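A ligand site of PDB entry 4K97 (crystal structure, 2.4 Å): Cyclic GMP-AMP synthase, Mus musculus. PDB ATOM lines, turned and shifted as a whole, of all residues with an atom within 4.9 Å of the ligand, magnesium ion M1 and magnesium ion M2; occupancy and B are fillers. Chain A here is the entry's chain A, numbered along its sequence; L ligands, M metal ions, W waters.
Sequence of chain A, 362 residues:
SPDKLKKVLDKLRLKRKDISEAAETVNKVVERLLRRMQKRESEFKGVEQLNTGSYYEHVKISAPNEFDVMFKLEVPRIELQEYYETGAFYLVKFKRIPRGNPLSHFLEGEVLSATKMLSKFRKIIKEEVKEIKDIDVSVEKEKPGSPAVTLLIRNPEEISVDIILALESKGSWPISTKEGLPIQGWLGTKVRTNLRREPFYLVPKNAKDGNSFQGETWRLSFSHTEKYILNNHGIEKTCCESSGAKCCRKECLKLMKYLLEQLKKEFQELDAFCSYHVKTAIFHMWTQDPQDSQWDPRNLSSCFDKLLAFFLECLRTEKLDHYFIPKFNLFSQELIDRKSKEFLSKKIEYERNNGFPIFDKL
Magnesium ion M1 is bound by OD1 of Asp 68 (2.1 Å), OE2 of Glu 66 (2.2 Å), OD2 of Asp 162 (2.2 Å), water W3 (2.4 Å) and O7 of the ligand (2.4 Å).
Magnesium ion M1 has five donor atoms within binding distance.
Slightly farther from magnesium ion M1 lies water W6 (2.7 Å).
Magnesium ion M2 is bound by OE1 of Glu 66 (1.9 Å), O4 of the ligand (2.1 Å), O2 of the ligand (2.1 Å), OD2 of Asp 68 (2.2 Å), O7 of the ligand (2.4 Å) and water W4 (2.4 Å).
The side-chain carboxylate (OE2) of Glu 226 lies within salt-bridge range of the side-chain amino group (NZ) of Lys 279.
OE1 of Glu 226 sits at hydrogen-bond distance from OH of Tyr 276 (2.7 Å).
N of Lys 60 sits at hydrogen-bond distance from O of Ser 54 (3.3 Å).
The side-chain carboxylate (OE2) of Glu 57 lies within salt-bridge range of the side-chain amino group (NZ) of Lys 279, 2.8 Å away.
SG of Cys 274 sits close to N of Tyr 276, 3.6 Å away.
O13 of the ligand sits at hydrogen-bond distance from OE2 of Glu 226, at 2.6 Å.
The side-chain hydroxyl (OG) of Ser 275 sits at hydrogen-bond distance from an oxygen (O3) of the ligand, 2.7 Å away.
N of Ser 54 lies close to O4 of the ligand (3.0 Å).
An oxygen (O1) of the ligand is in hydrogen-bond range of the side-chain hydroxyl of Ser 54 (2.7 Å).
The side-chain amino group (NZ) of Lys 257 is in salt-bridge range of an oxygen (O1) of the ligand (2.9 Å).
The side-chain amino group (NZ) of Lys 279 lies within hydrogen-bond range of an oxygen (O12) of the ligand (3.0 Å).
The side-chain hydroxyl (OG) of Ser 223 sits at hydrogen-bond distance from an oxygen (O13) of the ligand, 3.2 Å away.
The guanidinium group (NH2) of Arg 219 is in hydrogen-bond range of a nitrogen (N5) of the ligand, 3.4 Å away.
Within 4 Å of magnesium ion M2: Glu 66 and Asp 68.
The nearest printed residue that does not touch magnesium ion M2 is Ser 54 (4.2 Å).
Water W5 lies within hydrogen-bond range of an oxygen (O5) of the ligand (2.4 Å), the side-chain hydroxyl (OG) of Ser 275 (3.2 Å) and the backbone NH (N) of Tyr 276 (3.4 Å).
Water W8 lies within hydrogen-bond range of O8 of the ligand (2.5 Å), OG of Ser 275 (3.2 Å), N of Tyr 276 (3.5 Å) and SG of Cys 274 (3.7 Å).
Water W7 lies within hydrogen-bond range of an oxygen (O1) of the ligand and the side-chain amino group of Lys 60.
Gly 53 touches the ligand (CA to O4, 3.7 Å).
Tyr 276 touches the ligand.
Hydrophobic or aromatic side chains that line the ligand: Tyr 276.
11 residues have an atom within 4 Å of the ligand: Gly 53, Ser 54, Glu 66, Asp 68, Arg 219, Ser 223, Glu 226, Lys 257, Ser 275, Tyr 276 and Lys 279.
The nearest printed residue that does not touch the ligand is Lys 60 (4.2 Å).
The nearest printed residue that does not touch magnesium ion M1 is Gly 53 (7.2 Å).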
ATOM      1  N   GLY A  53      27.899  -3.776 -27.268  1.00  0.00           N
ATOM      2  CA  GLY A  53      28.734  -3.699 -26.067  1.00  0.00           C
ATOM      3  C   GLY A  53      28.786  -2.382 -25.311  1.00  0.00           C
ATOM      4  O   GLY A  53      28.074  -1.415 -25.643  1.00  0.00           O
ATOM      5  N   SER A  54      29.646  -2.355 -24.293  1.00  0.00           N
ATOM      6  CA  SER A  54      29.783  -1.248 -23.343  1.00  0.00           C
ATOM      7  C   SER A  54      29.721   0.169 -23.925  1.00  0.00           C
ATOM      8  O   SER A  54      28.886   0.968 -23.504  1.00  0.00           O
ATOM      9  CB  SER A  54      31.076  -1.419 -22.545  1.00  0.00           C
ATOM     10  OG  SER A  54      30.777  -1.631 -21.182  1.00  0.00           O
ATOM     11  N   GLU A  57      26.441   1.038 -25.490  1.00  0.00           N
ATOM     12  CA  GLU A  57      25.337   1.071 -24.541  1.00  0.00           C
ATOM     13  C   GLU A  57      25.523   2.214 -23.537  1.00  0.00           C
ATOM     14  O   GLU A  57      24.696   2.383 -22.640  1.00  0.00           O
ATOM     15  CB  GLU A  57      25.235  -0.253 -23.787  1.00  0.00           C
ATOM     16  CG  GLU A  57      24.997  -1.457 -24.679  1.00  0.00           C
ATOM     17  CD  GLU A  57      25.316  -2.775 -23.984  1.00  0.00           C
ATOM     18  OE1 GLU A  57      26.273  -2.821 -23.178  1.00  0.00           O
ATOM     19  OE2 GLU A  57      24.617  -3.770 -24.249  1.00  0.00           O
ATOM     20  N   LYS A  60      30.443   2.048 -20.835  1.00  0.00           N
ATOM     21  CA  LYS A  60      31.901   1.931 -20.813  1.00  0.00           C
ATOM     22  C   LYS A  60      32.442   2.865 -19.737  1.00  0.00           C
ATOM     23  O   LYS A  60      31.991   4.010 -19.616  1.00  0.00           O
ATOM     24  CB  LYS A  60      32.483   2.335 -22.180  1.00  0.00           C
ATOM     25  CG  LYS A  60      34.010   2.194 -22.306  1.00  0.00           C
ATOM     26  CD  LYS A  60      34.399   0.716 -22.410  1.00  0.00           C
ATOM     27  CE  LYS A  60      35.906   0.552 -22.608  1.00  0.00           C
ATOM     28  NZ  LYS A  60      36.671   0.761 -21.354  1.00  0.00           N
ATOM     29  N   GLU A  66      38.031   0.160 -25.484  1.00  0.00           N
ATOM     30  CA  GLU A  66      37.594  -1.172 -25.937  1.00  0.00           C
ATOM     31  C   GLU A  66      36.276  -1.066 -26.711  1.00  0.00           C
ATOM     32  O   GLU A  66      35.275  -0.566 -26.189  1.00  0.00           O
ATOM     33  CB  GLU A  66      37.463  -2.156 -24.755  1.00  0.00           C
ATOM     34  CG  GLU A  66      37.641  -3.651 -25.113  1.00  0.00           C
ATOM     35  CD  GLU A  66      36.322  -4.382 -25.397  1.00  0.00           C
ATOM     36  OE1 GLU A  66      35.241  -3.777 -25.251  1.00  0.00           O
ATOM     37  OE2 GLU A  66      36.374  -5.583 -25.759  1.00  0.00           O
ATOM     38  N   ASP A  68      33.400  -3.122 -29.266  1.00  0.00           N
ATOM     39  CA  ASP A  68      32.899  -4.378 -29.828  1.00  0.00           C
ATOM     40  C   ASP A  68      32.059  -4.120 -31.071  1.00  0.00           C
ATOM     41  O   ASP A  68      31.199  -3.235 -31.073  1.00  0.00           O
ATOM     42  CB  ASP A  68      32.049  -5.123 -28.806  1.00  0.00           C
ATOM     43  CG  ASP A  68      32.793  -5.374 -27.523  1.00  0.00           C
ATOM     44  OD1 ASP A  68      33.522  -6.382 -27.431  1.00  0.00           O
ATOM     45  OD2 ASP A  68      32.654  -4.530 -26.612  1.00  0.00           O
ATOM     46  N   ASP A 162      37.172  -5.614 -30.841  1.00  0.00           N
ATOM     47  CA  ASP A 162      36.763  -6.993 -31.147  1.00  0.00           C
ATOM     48  C   ASP A 162      35.802  -7.026 -32.324  1.00  0.00           C
ATOM     49  O   ASP A 162      34.665  -6.527 -32.214  1.00  0.00           O
ATOM     50  CB  ASP A 162      36.091  -7.652 -29.930  1.00  0.00           C
ATOM     51  CG  ASP A 162      37.054  -7.872 -28.767  1.00  0.00           C
ATOM     52  OD1 ASP A 162      38.257  -8.092 -29.016  1.00  0.00           O
ATOM     53  OD2 ASP A 162      36.606  -7.843 -27.599  1.00  0.00           O
ATOM     54  N   LYS A 205      31.996 -18.859 -31.037  1.00  0.00           N
ATOM     55  CA  LYS A 205      32.621 -19.171 -29.762  1.00  0.00           C
ATOM     56  C   LYS A 205      32.404 -20.664 -29.496  1.00  0.00           C
ATOM     57  O   LYS A 205      31.256 -21.109 -29.409  1.00  0.00           O
ATOM     58  CB  LYS A 205      31.996 -18.301 -28.668  1.00  0.00           C
ATOM     59  CG  LYS A 205      32.086 -18.842 -27.254  1.00  0.00           C
ATOM     60  CD  LYS A 205      33.473 -18.707 -26.681  1.00  0.00           C
ATOM     61  CE  LYS A 205      33.461 -18.714 -25.154  1.00  0.00           C
ATOM     62  NZ  LYS A 205      32.877 -17.463 -24.593  1.00  0.00           N
ATOM     63  N   ARG A 219      27.718 -20.282 -30.541  1.00  0.00           N
ATOM     64  CA  ARG A 219      26.994 -19.778 -29.376  1.00  0.00           C
ATOM     65  C   ARG A 219      25.926 -18.741 -29.688  1.00  0.00           C
ATOM     66  O   ARG A 219      26.083 -17.907 -30.525  1.00  0.00           O
ATOM     67  CB  ARG A 219      27.926 -19.240 -28.305  1.00  0.00           C
ATOM     68  CG  ARG A 219      27.500 -19.674 -26.927  1.00  0.00           C
ATOM     69  CD  ARG A 219      27.793 -18.706 -25.809  1.00  0.00           C
ATOM     70  NE  ARG A 219      27.647 -17.375 -26.311  1.00  0.00           N
ATOM     71  CZ  ARG A 219      28.450 -16.365 -26.048  1.00  0.00           C
ATOM     72  NH1 ARG A 219      29.479 -16.545 -25.242  1.00  0.00           N
ATOM     73  NH2 ARG A 219      28.210 -15.171 -26.585  1.00  0.00           N
ATOM     74  N   SER A 223      23.442  -9.637 -28.014  1.00  0.00           N
ATOM     75  CA  SER A 223      23.986  -8.285 -27.979  1.00  0.00           C
ATOM     76  C   SER A 223      22.993  -7.231 -28.481  1.00  0.00           C
ATOM     77  O   SER A 223      22.875  -6.168 -27.882  1.00  0.00           O
ATOM     78  CB  SER A 223      25.301  -8.195 -28.747  1.00  0.00           C
ATOM     79  OG  SER A 223      26.282  -9.060 -28.204  1.00  0.00           O
ATOM     80  N   GLU A 226      20.153  -6.873 -25.826  1.00  0.00           N
ATOM     81  CA  GLU A 226      20.698  -6.224 -24.627  1.00  0.00           C
ATOM     82  C   GLU A 226      20.867  -4.737 -24.881  1.00  0.00           C
ATOM     83  O   GLU A 226      20.647  -3.920 -24.001  1.00  0.00           O
ATOM     84  CB  GLU A 226      22.028  -6.854 -24.233  1.00  0.00           C
ATOM     85  CG  GLU A 226      21.896  -8.322 -23.828  1.00  0.00           C
ATOM     86  CD  GLU A 226      23.237  -9.051 -23.787  1.00  0.00           C
ATOM     87  OE1 GLU A 226      23.215 -10.296 -23.749  1.00  0.00           O
ATOM     88  OE2 GLU A 226      24.306  -8.399 -23.790  1.00  0.00           O
ATOM     89  N   LYS A 257      30.767  -2.852 -12.317  1.00  0.00           N
ATOM     90  CA  LYS A 257      31.815  -3.180 -13.269  1.00  0.00           C
ATOM     91  C   LYS A 257      33.160  -2.665 -12.781  1.00  0.00           C
ATOM     92  O   LYS A 257      34.175  -3.347 -12.920  1.00  0.00           O
ATOM     93  CB  LYS A 257      31.517  -2.622 -14.659  1.00  0.00           C
ATOM     94  CG  LYS A 257      30.334  -3.243 -15.337  1.00  0.00           C
ATOM     95  CD  LYS A 257      30.002  -2.501 -16.627  1.00  0.00           C
ATOM     96  CE  LYS A 257      31.139  -2.622 -17.618  1.00  0.00           C
ATOM     97  NZ  LYS A 257      30.723  -2.014 -18.899  1.00  0.00           N
ATOM     98  N   CYS A 274      33.982 -12.022 -15.745  1.00  0.00           N
ATOM     99  CA  CYS A 274      33.925 -11.012 -16.773  1.00  0.00           C
ATOM    100  C   CYS A 274      32.825 -10.035 -16.503  1.00  0.00           C
ATOM    101  O   CYS A 274      32.062 -10.211 -15.601  1.00  0.00           O
ATOM    102  CB  CYS A 274      33.758 -11.634 -18.143  1.00  0.00           C
ATOM    103  SG  CYS A 274      32.251 -12.514 -18.351  1.00  0.00           S
ATOM    104  N   SER A 275      32.794  -8.973 -17.254  1.00  0.00           N
ATOM    105  CA  SER A 275      31.766  -7.976 -17.101  1.00  0.00           C
ATOM    106  C   SER A 275      30.381  -8.504 -17.393  1.00  0.00           C
ATOM    107  O   SER A 275      29.470  -8.003 -16.851  1.00  0.00           O
ATOM    108  CB  SER A 275      32.081  -6.706 -17.846  1.00  0.00           C
ATOM    109  OG  SER A 275      32.250  -6.901 -19.198  1.00  0.00           O
ATOM    110  N   TYR A 276      30.250  -9.475 -18.273  1.00  0.00           N
ATOM    111  CA  TYR A 276      28.936 -10.071 -18.541  1.00  0.00           C
ATOM    112  C   TYR A 276      28.251 -10.666 -17.313  1.00  0.00           C
ATOM    113  O   TYR A 276      27.036 -10.574 -17.169  1.00  0.00           O
ATOM    114  CB  TYR A 276      29.034 -11.150 -19.617  1.00  0.00           C
ATOM    115  CG  TYR A 276      27.695 -11.440 -20.253  1.00  0.00           C
ATOM    116  CD1 TYR A 276      27.066 -10.486 -21.030  1.00  0.00           C
ATOM    117  CD2 TYR A 276      27.065 -12.669 -20.076  1.00  0.00           C
ATOM    118  CE1 TYR A 276      25.844 -10.728 -21.621  1.00  0.00           C
ATOM    119  CE2 TYR A 276      25.841 -12.924 -20.664  1.00  0.00           C
ATOM    120  CZ  TYR A 276      25.235 -11.951 -21.442  1.00  0.00           C
ATOM    121  OH  TYR A 276      24.014 -12.179 -22.037  1.00  0.00           O
ATOM    122  N   LYS A 279      26.663  -7.758 -15.813  1.00  0.00           N
ATOM    123  CA  LYS A 279      25.555  -7.309 -16.669  1.00  0.00           C
ATOM    124  C   LYS A 279      24.336  -8.217 -16.468  1.00  0.00           C
ATOM    125  O   LYS A 279      23.207  -7.741 -16.275  1.00  0.00           O
ATOM    126  CB  LYS A 279      26.019  -7.284 -18.136  1.00  0.00           C
ATOM    127  CG  LYS A 279      25.141  -6.472 -19.097  1.00  0.00           C
ATOM    128  CD  LYS A 279      25.743  -6.533 -20.520  1.00  0.00           C
ATOM    129  CE  LYS A 279      24.828  -5.929 -21.568  1.00  0.00           C
ATOM    130  NZ  LYS A 279      25.346  -6.157 -22.962  1.00  0.00           N
ATOM    131  N   HIS A 322      21.633 -17.410 -17.009  1.00  0.00           N
ATOM    132  CA  HIS A 322      21.701 -16.586 -18.214  1.00  0.00           C
ATOM    133  C   HIS A 322      20.335 -15.908 -18.384  1.00  0.00           C
ATOM    134  O   HIS A 322      19.306 -16.575 -18.272  1.00  0.00           O
ATOM    135  CB  HIS A 322      22.032 -17.463 -19.423  1.00  0.00           C
ATOM    136  CG  HIS A 322      22.401 -16.690 -20.653  1.00  0.00           C
ATOM    137  ND1 HIS A 322      21.502 -15.879 -21.311  1.00  0.00           N
ATOM    138  CD2 HIS A 322      23.566 -16.620 -21.342  1.00  0.00           C
ATOM    139  CE1 HIS A 322      22.105 -15.339 -22.361  1.00  0.00           C
ATOM    140  NE2 HIS A 322      23.354 -15.769 -22.403  1.00  0.00           N
HETATM  141  P1  LIG L   1      33.247  -4.056 -21.075  1.00  0.00           P
HETATM  142  O1  LIG L   1      33.129  -2.708 -20.397  1.00  0.00           O
HETATM  143  O2  LIG L   1      33.775  -3.981 -22.488  1.00  0.00           O
HETATM  144  O3  LIG L   1      33.960  -5.094 -20.245  1.00  0.00           O
HETATM  145  P2  LIG L   1      31.151  -5.311 -22.528  1.00  0.00           P
HETATM  146  O4  LIG L   1      31.544  -4.552 -23.770  1.00  0.00           O
HETATM  147  O5  LIG L   1      29.693  -5.614 -22.262  1.00  0.00           O
HETATM  148  O6  LIG L   1      31.732  -4.595 -21.190  1.00  0.00           O
HETATM  149  P3  LIG L   1      32.740  -7.537 -23.540  1.00  0.00           P
HETATM  150  O7  LIG L   1      33.527  -6.556 -24.387  1.00  0.00           O
HETATM  151  O8  LIG L   1      33.423  -8.651 -22.791  1.00  0.00           O
HETATM  152  O9  LIG L   1      31.926  -6.736 -22.404  1.00  0.00           O
HETATM  153  O10 LIG L   1      31.629  -8.265 -24.459  1.00  0.00           O
HETATM  154  C1  LIG L   1      30.916  -7.543 -25.465  1.00  0.00           C
HETATM  155  C2  LIG L   1      29.515  -8.158 -25.619  1.00  0.00           C
HETATM  156  O11 LIG L   1      29.558  -9.536 -26.018  1.00  0.00           O
HETATM  157  C3  LIG L   1      28.744  -8.112 -24.314  1.00  0.00           C
HETATM  158  O12 LIG L   1      28.011  -6.892 -24.180  1.00  0.00           O
HETATM  159  C4  LIG L   1      27.820  -9.320 -24.399  1.00  0.00           C
HETATM  160  O13 LIG L   1      26.564  -8.986 -25.000  1.00  0.00           O
HETATM  161  C5  LIG L   1      28.580 -10.303 -25.294  1.00  0.00           C
HETATM  162  N1  LIG L   1      29.250 -11.273 -24.387  1.00  0.00           N
HETATM  163  C6  LIG L   1      30.499 -11.144 -23.906  1.00  0.00           C
HETATM  164  N2  LIG L   1      30.824 -12.184 -23.097  1.00  0.00           N
HETATM  165  C7  LIG L   1      29.768 -13.009 -23.042  1.00  0.00           C
HETATM  166  C8  LIG L   1      29.461 -14.291 -22.367  1.00  0.00           C
HETATM  167  N3  LIG L   1      30.382 -14.891 -21.561  1.00  0.00           N
HETATM  168  N4  LIG L   1      28.229 -14.828 -22.569  1.00  0.00           N
HETATM  169  C9  LIG L   1      27.313 -14.219 -23.365  1.00  0.00           C
HETATM  170  N5  LIG L   1      27.532 -13.050 -24.007  1.00  0.00           N
HETATM  171  C10 LIG L   1      28.719 -12.412 -23.895  1.00  0.00           C
HETATM  172 MG    MG M   1      35.014  -7.242 -26.184  1.00  0.00          MG
HETATM  173 MG    MG M   2      33.468  -4.194 -24.576  1.00  0.00          MG
HETATM  174  O   HOH W   1      29.137 -12.793 -27.678  1.00  0.00           O
HETATM  175  O   HOH W   2      33.196 -12.673 -22.304  1.00  0.00           O
HETATM  176  O   HOH W   3      36.472  -7.609 -24.287  1.00  0.00           O
HETATM  177  O   HOH W   4      33.078  -1.827 -24.934  1.00  0.00           O
HETATM  178  O   HOH W   5      29.224  -6.834 -20.238  1.00  0.00           O
HETATM  179  O   HOH W   6      34.096  -9.796 -26.504  1.00  0.00           O
HETATM  180  O   HOH W   7      34.655  -0.826 -19.012  1.00  0.00           O
HETATM  181  O   HOH W   8      32.707  -9.696 -20.689  1.00  0.00           O
